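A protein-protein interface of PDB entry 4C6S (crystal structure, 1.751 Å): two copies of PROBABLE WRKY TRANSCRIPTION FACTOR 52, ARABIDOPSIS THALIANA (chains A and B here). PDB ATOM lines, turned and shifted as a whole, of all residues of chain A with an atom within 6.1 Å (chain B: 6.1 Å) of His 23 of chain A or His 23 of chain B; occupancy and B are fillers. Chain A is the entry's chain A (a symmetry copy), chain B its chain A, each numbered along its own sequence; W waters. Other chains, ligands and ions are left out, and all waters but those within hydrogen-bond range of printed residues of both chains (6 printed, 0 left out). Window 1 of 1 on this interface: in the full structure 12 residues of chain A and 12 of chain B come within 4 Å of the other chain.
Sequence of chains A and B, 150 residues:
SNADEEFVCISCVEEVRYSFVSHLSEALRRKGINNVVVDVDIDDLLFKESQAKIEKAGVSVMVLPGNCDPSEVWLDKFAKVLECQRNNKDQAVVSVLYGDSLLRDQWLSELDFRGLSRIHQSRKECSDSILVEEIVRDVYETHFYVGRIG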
ATOM      1  N   TYR A  18      16.891  -8.844  11.523  1.00  0.00           N
ATOM      2  CA  TYR A  18      17.590  -9.308  10.320  1.00  0.00           C
ATOM      3  C   TYR A  18      18.983  -9.844  10.638  1.00  0.00           C
ATOM      4  O   TYR A  18      19.728 -10.234   9.730  1.00  0.00           O
ATOM      5  CB  TYR A  18      17.674  -8.187   9.291  1.00  0.00           C
ATOM      6  CG  TYR A  18      16.328  -7.796   8.740  1.00  0.00           C
ATOM      7  CD1 TYR A  18      15.647  -8.647   7.887  1.00  0.00           C
ATOM      8  CD2 TYR A  18      15.721  -6.600   9.109  1.00  0.00           C
ATOM      9  CE1 TYR A  18      14.404  -8.309   7.383  1.00  0.00           C
ATOM     10  CE2 TYR A  18      14.473  -6.249   8.605  1.00  0.00           C
ATOM     11  CZ  TYR A  18      13.824  -7.112   7.746  1.00  0.00           C
ATOM     12  OH  TYR A  18      12.587  -6.783   7.237  1.00  0.00           O
ATOM     13  N   SER A  19      19.332  -9.838  11.918  1.00  0.00           N
ATOM     14  CA  SER A  19      20.617 -10.368  12.351  1.00  0.00           C
ATOM     15  C   SER A  19      20.379 -11.631  13.166  1.00  0.00           C
ATOM     16  O   SER A  19      20.011 -12.643  12.598  1.00  0.00           O
ATOM     17  CB  SER A  19      21.442  -9.302  13.085  1.00  0.00           C
ATOM     18  OG  SER A  19      20.705  -8.773  14.173  1.00  0.00           O
ATOM     19  N   PHE A  20      20.542 -11.582  14.484  1.00  0.00           N
ATOM     20  CA  PHE A  20      20.381 -12.772  15.336  1.00  0.00           C
ATOM     21  C   PHE A  20      19.108 -13.589  15.080  1.00  0.00           C
ATOM     22  O   PHE A  20      19.163 -14.814  14.961  1.00  0.00           O
ATOM     23  CB  PHE A  20      20.410 -12.356  16.817  1.00  0.00           C
ATOM     24  CG  PHE A  20      20.175 -13.494  17.769  1.00  0.00           C
ATOM     25  CD1 PHE A  20      21.183 -14.428  18.025  1.00  0.00           C
ATOM     26  CD2 PHE A  20      18.952 -13.631  18.414  1.00  0.00           C
ATOM     27  CE1 PHE A  20      20.961 -15.478  18.933  1.00  0.00           C
ATOM     28  CE2 PHE A  20      18.718 -14.680  19.321  1.00  0.00           C
ATOM     29  CZ  PHE A  20      19.732 -15.608  19.567  1.00  0.00           C
ATOM     30  N   VAL A  21      17.963 -12.922  15.013  1.00  0.00           N
ATOM     31  CA  VAL A  21      16.696 -13.633  14.854  1.00  0.00           C
ATOM     32  C   VAL A  21      16.633 -14.386  13.525  1.00  0.00           C
ATOM     33  O   VAL A  21      16.019 -15.459  13.427  1.00  0.00           O
ATOM     34  CB  VAL A  21      15.513 -12.668  15.027  1.00  0.00           C
ATOM     35  CG1 VAL A  21      14.194 -13.294  14.581  1.00  0.00           C
ATOM     36  CG2 VAL A  21      15.433 -12.216  16.511  1.00  0.00           C
ATOM     37  N   SER A  22      17.288 -13.851  12.497  1.00  0.00           N
ATOM     38  CA  SER A  22      17.208 -14.510  11.189  1.00  0.00           C
ATOM     39  C   SER A  22      17.945 -15.855  11.278  1.00  0.00           C
ATOM     40  O   SER A  22      17.546 -16.838  10.649  1.00  0.00           O
ATOM     41  CB  SER A  22      17.764 -13.631  10.063  1.00  0.00           C
ATOM     42  OG  SER A  22      19.179 -13.567  10.082  1.00  0.00           O
ATOM     43  N   HIS A  23      19.004 -15.900  12.075  1.00  0.00           N
ATOM     44  CA  HIS A  23      19.739 -17.149  12.243  1.00  0.00           C
ATOM     45  C   HIS A  23      18.925 -18.125  13.063  1.00  0.00           C
ATOM     46  O   HIS A  23      18.948 -19.329  12.796  1.00  0.00           O
ATOM     47  CB  HIS A  23      21.100 -16.916  12.909  1.00  0.00           C
ATOM     48  CG  HIS A  23      21.978 -15.976  12.152  1.00  0.00           C
ATOM     49  ND1 HIS A  23      22.567 -16.301  10.952  1.00  0.00           N
ATOM     50  CD2 HIS A  23      22.372 -14.706  12.432  1.00  0.00           C
ATOM     51  CE1 HIS A  23      23.289 -15.278  10.523  1.00  0.00           C
ATOM     52  NE2 HIS A  23      23.190 -14.302  11.416  1.00  0.00           N
ATOM     53  N   LEU A  24      18.227 -17.610  14.072  1.00  0.00           N
ATOM     54  CA  LEU A  24      17.382 -18.450  14.924  1.00  0.00           C
ATOM     55  C   LEU A  24      16.245 -19.055  14.109  1.00  0.00           C
ATOM     56  O   LEU A  24      15.977 -20.254  14.201  1.00  0.00           O
ATOM     57  CB  LEU A  24      16.819 -17.643  16.109  1.00  0.00           C
ATOM     58  CG  LEU A  24      15.869 -18.396  17.060  1.00  0.00           C
ATOM     59  CD1 LEU A  24      16.537 -19.642  17.658  1.00  0.00           C
ATOM     60  CD2 LEU A  24      15.405 -17.464  18.177  1.00  0.00           C
ATOM     61  N   SER A  25      15.584 -18.230  13.298  1.00  0.00           N
ATOM     62  CA  SER A  25      14.530 -18.711  12.414  1.00  0.00           C
ATOM     63  C   SER A  25      15.027 -19.782  11.452  1.00  0.00           C
ATOM     64  O   SER A  25      14.350 -20.807  11.234  1.00  0.00           O
ATOM     65  CB  SER A  25      13.945 -17.542  11.606  1.00  0.00           C
ATOM     66  OG  SER A  25      12.901 -17.966  10.751  1.00  0.00           O
ATOM     67  N   GLU A  26      16.191 -19.546  10.852  1.00  0.00           N
ATOM     68  CA  GLU A  26      16.702 -20.496   9.870  1.00  0.00           C
ATOM     69  C   GLU A  26      17.105 -21.796  10.563  1.00  0.00           C
ATOM     70  O   GLU A  26      16.957 -22.881   9.993  1.00  0.00           O
ATOM     71  CB  GLU A  26      17.869 -19.891   9.081  1.00  0.00           C
ATOM     72  CG  GLU A  26      18.643 -20.877   8.211  1.00  0.00           C
ATOM     73  CD  GLU A  26      17.835 -21.436   7.046  1.00  0.00           C
ATOM     74  OE1 GLU A  26      16.718 -20.934   6.769  1.00  0.00           O
ATOM     75  OE2 GLU A  26      18.334 -22.381   6.398  1.00  0.00           O
ATOM     76  N   ALA A  27      17.609 -21.701  11.787  1.00  0.00           N
ATOM     77  CA  ALA A  27      18.009 -22.912  12.505  1.00  0.00           C
ATOM     78  C   ALA A  27      16.790 -23.753  12.887  1.00  0.00           C
ATOM     79  O   ALA A  27      16.819 -24.985  12.812  1.00  0.00           O
ATOM     80  CB  ALA A  27      18.846 -22.552  13.734  1.00  0.00           C
ATOM     81  N   LEU A  28      15.712 -23.096  13.309  1.00  0.00           N
ATOM     82  CA  LEU A  28      14.466 -23.830  13.569  1.00  0.00           C
ATOM     83  C   LEU A  28      13.964 -24.520  12.305  1.00  0.00           C
ATOM     84  O   LEU A  28      13.558 -25.688  12.342  1.00  0.00           O
ATOM     85  CB  LEU A  28      13.386 -22.895  14.121  1.00  0.00           C
ATOM     86  CG  LEU A  28      13.607 -22.405  15.551  1.00  0.00           C
ATOM     87  CD1 LEU A  28      12.654 -21.252  15.832  1.00  0.00           C
ATOM     88  CD2 LEU A  28      13.392 -23.549  16.539  1.00  0.00           C
ATOM     89  N   ARG A  30      15.689 -25.533   9.719  1.00  0.00           N
ATOM     90  CA  ARG A  30      16.577 -26.643   9.392  1.00  0.00           C
ATOM     91  C   ARG A  30      16.248 -27.870  10.218  1.00  0.00           C
ATOM     92  O   ARG A  30      16.511 -28.995   9.802  1.00  0.00           O
ATOM     93  CB  ARG A  30      18.044 -26.270   9.629  1.00  0.00           C
ATOM     94  CG  ARG A  30      18.661 -25.377   8.571  1.00  0.00           C
ATOM     95  CD  ARG A  30      20.186 -25.424   8.665  1.00  0.00           C
ATOM     96  NE  ARG A  30      20.651 -25.209  10.035  1.00  0.00           N
ATOM     97  CZ  ARG A  30      20.985 -24.021  10.530  1.00  0.00           C
ATOM     98  NH1 ARG A  30      20.910 -22.942   9.764  1.00  0.00           N
ATOM     99  NH2 ARG A  30      21.398 -23.910  11.788  1.00  0.00           N
ATOM    100  N   ASP A 128      27.039 -16.583  19.395  1.00  0.00           N
ATOM    101  CA  ASP A 128      25.601 -16.551  19.135  1.00  0.00           C
ATOM    102  C   ASP A 128      25.147 -17.814  18.417  1.00  0.00           C
ATOM    103  O   ASP A 128      23.992 -18.203  18.521  1.00  0.00           O
ATOM    104  CB  ASP A 128      25.212 -15.321  18.297  1.00  0.00           C
ATOM    105  CG  ASP A 128      25.252 -14.029  19.085  1.00  0.00           C
ATOM    106  OD1 ASP A 128      25.411 -14.098  20.315  1.00  0.00           O
ATOM    107  OD2 ASP A 128      25.124 -12.941  18.472  1.00  0.00           O
ATOM    108  N   SER A 129      26.044 -18.453  17.670  1.00  0.00           N
ATOM    109  CA  SER A 129      25.662 -19.663  16.964  1.00  0.00           C
ATOM    110  C   SER A 129      25.369 -20.751  17.988  1.00  0.00           C
ATOM    111  O   SER A 129      24.448 -21.547  17.809  1.00  0.00           O
ATOM    112  CB  SER A 129      26.731 -20.124  15.969  1.00  0.00           C
ATOM    113  OG  SER A 129      27.963 -20.370  16.619  1.00  0.00           O
ATOM    114  N   ILE A 130      26.139 -20.770  19.071  1.00  0.00           N
ATOM    115  CA  ILE A 130      25.884 -21.724  20.153  1.00  0.00           C
ATOM    116  C   ILE A 130      24.552 -21.392  20.835  1.00  0.00           C
ATOM    117  O   ILE A 130      23.740 -22.288  21.086  1.00  0.00           O
ATOM    118  CB  ILE A 130      27.032 -21.744  21.178  1.00  0.00           C
ATOM    119  CG1 ILE A 130      28.314 -22.247  20.525  1.00  0.00           C
ATOM    120  CG2 ILE A 130      26.676 -22.665  22.350  1.00  0.00           C
ATOM    121  CD1 ILE A 130      28.261 -23.716  20.166  1.00  0.00           C
ATOM    122  N   VAL A 132      21.948 -19.894  19.575  1.00  0.00           N
ATOM    123  CA  VAL A 132      20.883 -20.372  18.689  1.00  0.00           C
ATOM    124  C   VAL A 132      20.675 -21.878  18.836  1.00  0.00           C
ATOM    125  O   VAL A 132      19.534 -22.338  18.971  1.00  0.00           O
ATOM    126  CB  VAL A 132      21.155 -20.025  17.216  1.00  0.00           C
ATOM    127  CG1 VAL A 132      20.215 -20.809  16.278  1.00  0.00           C
ATOM    128  CG2 VAL A 132      20.972 -18.532  17.002  1.00  0.00           C
ATOM    129  N   TYR B  18      31.844 -13.126  17.679  1.00  0.00           N
ATOM    130  CA  TYR B  18      30.951 -14.048  18.388  1.00  0.00           C
ATOM    131  C   TYR B  18      29.503 -13.910  17.929  1.00  0.00           C
ATOM    132  O   TYR B  18      28.609 -14.583  18.459  1.00  0.00           O
ATOM    133  CB  TYR B  18      31.054 -13.831  19.893  1.00  0.00           C
ATOM    134  CG  TYR B  18      32.401 -14.211  20.449  1.00  0.00           C
ATOM    135  CD1 TYR B  18      32.778 -15.540  20.525  1.00  0.00           C
ATOM    136  CD2 TYR B  18      33.312 -13.239  20.851  1.00  0.00           C
ATOM    137  CE1 TYR B  18      34.017 -15.905  21.020  1.00  0.00           C
ATOM    138  CE2 TYR B  18      34.559 -13.596  21.353  1.00  0.00           C
ATOM    139  CZ  TYR B  18      34.901 -14.930  21.430  1.00  0.00           C
ATOM    140  OH  TYR B  18      36.132 -15.302  21.923  1.00  0.00           O
ATOM    141  N   SER B  19      29.278 -13.026  16.966  1.00  0.00           N
ATOM    142  CA  SER B  19      27.945 -12.838  16.411  1.00  0.00           C
ATOM    143  C   SER B  19      27.937 -13.331  14.971  1.00  0.00           C
ATOM    144  O   SER B  19      27.997 -14.527  14.753  1.00  0.00           O
ATOM    145  CB  SER B  19      27.472 -11.386  16.573  1.00  0.00           C
ATOM    146  OG  SER B  19      28.407 -10.496  15.990  1.00  0.00           O
ATOM    147  N   PHE B  20      27.907 -12.436  13.989  1.00  0.00           N
ATOM    148  CA  PHE B  20      27.846 -12.832  12.572  1.00  0.00           C
ATOM    149  C   PHE B  20      28.853 -13.910  12.153  1.00  0.00           C
ATOM    150  O   PHE B  20      28.491 -14.883  11.490  1.00  0.00           O
ATOM    151  CB  PHE B  20      28.048 -11.596  11.679  1.00  0.00           C
ATOM    152  CG  PHE B  20      28.080 -11.910  10.211  1.00  0.00           C
ATOM    153  CD1 PHE B  20      26.901 -12.201   9.519  1.00  0.00           C
ATOM    154  CD2 PHE B  20      29.284 -11.910   9.517  1.00  0.00           C
ATOM    155  CE1 PHE B  20      26.938 -12.473   8.140  1.00  0.00           C
ATOM    156  CE2 PHE B  20      29.332 -12.185   8.139  1.00  0.00           C
ATOM    157  CZ  PHE B  20      28.148 -12.476   7.458  1.00  0.00           C
ATOM    158  N   VAL B  21      30.117 -13.735  12.521  1.00  0.00           N
ATOM    159  CA  VAL B  21      31.153 -14.673  12.093  1.00  0.00           C
ATOM    160  C   VAL B  21      30.914 -16.074  12.655  1.00  0.00           C
ATOM    161  O   VAL B  21      31.237 -17.084  12.012  1.00  0.00           O
ATOM    162  CB  VAL B  21      32.546 -14.134  12.455  1.00  0.00           C
ATOM    163  CG1 VAL B  21      33.629 -15.200  12.299  1.00  0.00           C
ATOM    164  CG2 VAL B  21      32.863 -12.896  11.573  1.00  0.00           C
ATOM    165  N   SER B  22      30.324 -16.154  13.846  1.00  0.00           N
ATOM    166  CA  SER B  22      30.126 -17.477  14.448  1.00  0.00           C
ATOM    167  C   SER B  22      29.094 -18.243  13.607  1.00  0.00           C
ATOM    168  O   SER B  22      29.184 -19.463  13.452  1.00  0.00           O
ATOM    169  CB  SER B  22      29.706 -17.385  15.919  1.00  0.00           C
ATOM    170  OG  SER B  22      28.357 -16.980  16.067  1.00  0.00           O
ATOM    171  N   HIS B  23      28.129 -17.523  13.051  1.00  0.00           N
ATOM    172  CA  HIS B  23      27.129 -18.170  12.208  1.00  0.00           C
ATOM    173  C   HIS B  23      27.748 -18.586  10.893  1.00  0.00           C
ATOM    174  O   HIS B  23      27.409 -19.644  10.355  1.00  0.00           O
ATOM    175  CB  HIS B  23      25.929 -17.251  11.952  1.00  0.00           C
ATOM    176  CG  HIS B  23      25.245 -16.806  13.201  1.00  0.00           C
ATOM    177  ND1 HIS B  23      24.493 -17.650  13.985  1.00  0.00           N
ATOM    178  CD2 HIS B  23      25.199 -15.590  13.806  1.00  0.00           C
ATOM    179  CE1 HIS B  23      24.007 -16.978  15.017  1.00  0.00           C
ATOM    180  NE2 HIS B  23      24.418 -15.721  14.919  1.00  0.00           N
ATOM    181  N   LEU B  24      28.636 -17.747  10.365  1.00  0.00           N
ATOM    182  CA  LEU B  24      29.321 -18.049   9.107  1.00  0.00           C
ATOM    183  C   LEU B  24      30.201 -19.284   9.267  1.00  0.00           C
ATOM    184  O   LEU B  24      30.175 -20.185   8.428  1.00  0.00           O
ATOM    185  CB  LEU B  24      30.164 -16.850   8.636  1.00  0.00           C
ATOM    186  CG  LEU B  24      30.981 -17.052   7.345  1.00  0.00           C
ATOM    187  CD1 LEU B  24      30.083 -17.446   6.163  1.00  0.00           C
ATOM    188  CD2 LEU B  24      31.754 -15.778   7.013  1.00  0.00           C
ATOM    189  N   SER B  25      30.970 -19.334  10.354  1.00  0.00           N
ATOM    190  CA  SER B  25      31.794 -20.498  10.652  1.00  0.00           C
ATOM    191  C   SER B  25      30.969 -21.772  10.779  1.00  0.00           C
ATOM    192  O   SER B  25      31.355 -22.836  10.255  1.00  0.00           O
ATOM    193  CB  SER B  25      32.575 -20.272  11.957  1.00  0.00           C
ATOM    194  OG  SER B  25      33.405 -21.373  12.269  1.00  0.00           O
ATOM    195  N   GLU B  26      29.851 -21.685  11.494  1.00  0.00           N
ATOM    196  CA  GLU B  26      29.040 -22.878  11.714  1.00  0.00           C
ATOM    197  C   GLU B  26      28.394 -23.318  10.402  1.00  0.00           C
ATOM    198  O   GLU B  26      28.222 -24.516  10.160  1.00  0.00           O
ATOM    199  CB  GLU B  26      27.992 -22.633  12.806  1.00  0.00           C
ATOM    200  CG  GLU B  26      26.928 -23.718  12.938  1.00  0.00           C
ATOM    201  CD  GLU B  26      27.471 -25.055  13.429  1.00  0.00           C
ATOM    202  OE1 GLU B  26      28.648 -25.126  13.859  1.00  0.00           O
ATOM    203  OE2 GLU B  26      26.702 -26.040  13.390  1.00  0.00           O
ATOM    204  N   ALA B  27      28.036 -22.363   9.551  1.00  0.00           N
ATOM    205  CA  ALA B  27      27.416 -22.722   8.275  1.00  0.00           C
ATOM    206  C   ALA B  27      28.422 -23.409   7.349  1.00  0.00           C
ATOM    207  O   ALA B  27      28.087 -24.367   6.645  1.00  0.00           O
ATOM    208  CB  ALA B  27      26.803 -21.486   7.614  1.00  0.00           C
ATOM    209  N   LEU B  28      29.660 -22.920   7.334  1.00  0.00           N
ATOM    210  CA  LEU B  28      30.707 -23.610   6.569  1.00  0.00           C
ATOM    211  C   LEU B  28      30.914 -25.031   7.080  1.00  0.00           C
ATOM    212  O   LEU B  28      31.024 -25.977   6.291  1.00  0.00           O
ATOM    213  CB  LEU B  28      32.027 -22.834   6.625  1.00  0.00           C
ATOM    214  CG  LEU B  28      32.057 -21.527   5.834  1.00  0.00           C
ATOM    215  CD1 LEU B  28      33.283 -20.726   6.249  1.00  0.00           C
ATOM    216  CD2 LEU B  28      32.071 -21.818   4.336  1.00  0.00           C
ATOM    217  N   ARG B  30      28.775 -26.971   8.616  1.00  0.00           N
ATOM    218  CA  ARG B  30      27.619 -27.784   8.258  1.00  0.00           C
ATOM    219  C   ARG B  30      27.709 -28.265   6.825  1.00  0.00           C
ATOM    220  O   ARG B  30      27.145 -29.297   6.473  1.00  0.00           O
ATOM    221  CB  ARG B  30      26.314 -27.001   8.433  1.00  0.00           C
ATOM    222  CG  ARG B  30      25.843 -26.842   9.866  1.00  0.00           C
ATOM    223  CD  ARG B  30      24.368 -26.447   9.895  1.00  0.00           C
ATOM    224  NE  ARG B  30      24.090 -25.322   9.001  1.00  0.00           N
ATOM    225  CZ  ARG B  30      24.100 -24.048   9.383  1.00  0.00           C
ATOM    226  NH1 ARG B  30      24.369 -23.738  10.643  1.00  0.00           N
ATOM    227  NH2 ARG B  30      23.838 -23.084   8.508  1.00  0.00           N
ATOM    228  N   ASP B 128      20.837 -11.526   7.622  1.00  0.00           N
ATOM    229  CA  ASP B 128      22.211 -12.015   7.720  1.00  0.00           C
ATOM    230  C   ASP B 128      22.279 -13.511   7.455  1.00  0.00           C
ATOM    231  O   ASP B 128      23.309 -14.019   7.032  1.00  0.00           O
ATOM    232  CB  ASP B 128      22.815 -11.714   9.102  1.00  0.00           C
ATOM    233  CG  ASP B 128      23.159 -10.252   9.295  1.00  0.00           C
ATOM    234  OD1 ASP B 128      23.097  -9.501   8.307  1.00  0.00           O
ATOM    235  OD2 ASP B 128      23.496  -9.854  10.436  1.00  0.00           O
ATOM    236  N   SER B 129      21.193 -14.232   7.718  1.00  0.00           N
ATOM    237  CA  SER B 129      21.205 -15.666   7.483  1.00  0.00           C
ATOM    238  C   SER B 129      21.311 -15.912   5.984  1.00  0.00           C
ATOM    239  O   SER B 129      21.991 -16.840   5.550  1.00  0.00           O
ATOM    240  CB  SER B 129      19.973 -16.366   8.065  1.00  0.00           C
ATOM    241  OG  SER B 129      18.780 -15.845   7.513  1.00  0.00           O
ATOM    242  N   ILE B 130      20.657 -15.065   5.196  1.00  0.00           N
ATOM    243  CA  ILE B 130      20.765 -15.166   3.739  1.00  0.00           C
ATOM    244  C   ILE B 130      22.191 -14.820   3.297  1.00  0.00           C
ATOM    245  O   ILE B 130      22.779 -15.530   2.476  1.00  0.00           O
ATOM    246  CB  ILE B 130      19.740 -14.264   3.028  1.00  0.00           C
ATOM    247  CG1 ILE B 130      18.322 -14.732   3.335  1.00  0.00           C
ATOM    248  CG2 ILE B 130      19.961 -14.310   1.512  1.00  0.00           C
ATOM    249  CD1 ILE B 130      17.983 -16.062   2.698  1.00  0.00           C
ATOM    250  N   VAL B 132      24.963 -15.123   4.983  1.00  0.00           N
ATOM    251  CA  VAL B 132      25.797 -16.288   5.284  1.00  0.00           C
ATOM    252  C   VAL B 132      25.644 -17.369   4.216  1.00  0.00           C
ATOM    253  O   VAL B 132      26.645 -17.907   3.726  1.00  0.00           O
ATOM    254  CB  VAL B 132      25.491 -16.878   6.671  1.00  0.00           C
ATOM    255  CG1 VAL B 132      26.127 -18.274   6.834  1.00  0.00           C
ATOM    256  CG2 VAL B 132      26.014 -15.945   7.749  1.00  0.00           C
HETATM  257  O   HOH W   1      18.108 -18.061   5.440  1.00  0.00           O
HETATM  258  O   HOH W   2      27.891 -23.471  16.799  1.00  0.00           O
HETATM  259  O   HOH W   3      15.828 -16.559   8.269  1.00  0.00           O
HETATM  260  O   HOH W   4      24.066 -13.281  16.021  1.00  0.00           O
HETATM  261  O   HOH W   5      24.222 -11.887  12.043  1.00  0.00           O
HETATM  262  O   HOH W   6      30.706 -21.153  15.330  1.00  0.00           O
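N of Asp 128 of chain B lies within hydrogen-bond range of O of Tyr 18 of chain A.
N of Ser 129 of chain B lies within hydrogen-bond range of OG of Ser 22 of chain A (3.2 Å).
The backbone carbonyl oxygen (O) of Tyr 18 of chain B sits at hydrogen-bond distance from the backbone NH (N) of Asp 128 of chain A (2.7 Å).
NH2 of Arg 30 of chain A sits close to NH1 of Arg 30 of chain B (3.2 Å).
The backbone NH (N) of Ser 129 of chain A is in hydrogen-bond range of the side-chain hydroxyl (OG) of Ser 22 of chain B, at 3.2 Å.
The backbone carbonyl oxygen of Tyr 18 of chain B is in hydrogen-bond range of the side-chain hydroxyl of Ser 22 of chain B (3.4 Å).
The side-chain hydroxyl (OG) of Ser 22 of chain B is in hydrogen-bond range of the backbone carbonyl oxygen (O) of Ser 19 of chain B.
The backbone carbonyl oxygen (O) of Tyr 18 of chain A is in hydrogen-bond range of the side-chain hydroxyl (OG) of Ser 22 of chain A (3.4 Å).
OG of Ser 22 of chain A sits at hydrogen-bond distance from O of Ser 19 of chain A (2.8 Å).
Among the printed residues, merely in contact across the chains: Ser 19 of chain A with Asp 128 of chain B (3.4 Å), Ser 22 of chain A with Asp 128 of chain B (3.6 Å), His 23 of chain A with His 23 of chain B (3.3 Å), His 23 of chain A with Asp 128 of chain B (3.5 Å), His 23 of chain A with Ser 129 of chain B (3.7 Å), His 23 of chain A with Val 132 of chain B (3.9 Å), Asp 128 of chain A with Ser 19 of chain B (3.4 Å), Asp 128 of chain A with Ser 22 of chain B (3.6 Å), Asp 128 of chain A with His 23 of chain B (3.5 Å), Ser 129 of chain A with His 23 of chain B (3.7 Å) and Val 132 of chain A with His 23 of chain B (3.9 Å).
His 23 of chain A touches just these residues of chain B: His 23 (3.3 Å), Asp 128 (3.5 Å), Ser 129 (3.7 Å) and Val 132 (3.9 Å).
Leu 24 of chain A touches none of the printed residues of chain B.
Ala 27 of chain A touches none of the printed residues of chain B.
Of the printed residues of chain A, Ser 22 of chain B touches Asp 128 (3.6 Å) and Ser 129 (3.2 Å).
Of the printed residues of chain A, His 23 of chain B touches His 23 (3.3 Å), Asp 128 (3.5 Å), Ser 129 (3.7 Å) and Val 132 (3.9 Å).
Of the printed residues of chain A, Asp 128 of chain B touches Tyr 18, Ser 19, Ser 22 and His 23.
Of the printed residues of chain A, Val 132 of chain B touches His 23.
The nearest residue of chain B that does not touch His 23 of chain A is Phe 20 of chain B (4.7 Å).
Of the 16 printed residues of chain B, 8 touch a printed residue of chain A.
Hydrophobic or aromatic side chains of chain B that line the printed part of chain A: His 23 and Val 132.
Ser 22 of chain A touches Asp 128 of chain B, and with the chains exchanged Asp 128 of chain A touches Ser 22 of chain B.
His 23 of chain B touches its own counterpart, His 23 of chain A.
His 23 of chain A touches Asp 128 of chain B, and with the chains exchanged Asp 128 of chain A touches His 23 of chain B.
His 23 of chain A touches Ser 129 of chain B, and with the chains exchanged Ser 129 of chain A touches His 23 of chain B.
Positions printed for both chains: 18, 19, 20, 21, 22, 23, 24, 25, 26, 27, 28, 30, 128, 129, 130 and 132.
Water W5 bridges the side-chain carboxylate of Asp 128 of chain B (2.7 Å) and a ring nitrogen (NE2) of His 23 of chain A (2.7 Å).
Water W4 lies within hydrogen-bond range of OD2 of Asp 128 of chain A (2.7 Å) and NE2 of His 23 of chain B (2.7 Å).
Water W3 lies within hydrogen-bond range of the backbone carbonyl oxygen (O) of Ser 22 of chain A and the side-chain hydroxyl (OG) of Ser 129 of chain B.
Water W6 lies within hydrogen-bond range of the backbone carbonyl oxygen of Ser 22 of chain B (2.9 Å) and the side-chain hydroxyl of Ser 129 of chain A (3.1 Å).
Water W2 bridges OG of Ser 129 of chain A (3.1 Å) and OE1 of Glu 26 of chain B (3.5 Å).
Water W1 bridges the side-chain hydroxyl of Ser 129 of chain B (3.1 Å) and the side-chain carboxylate of Glu 26 of chain A (3.5 Å).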
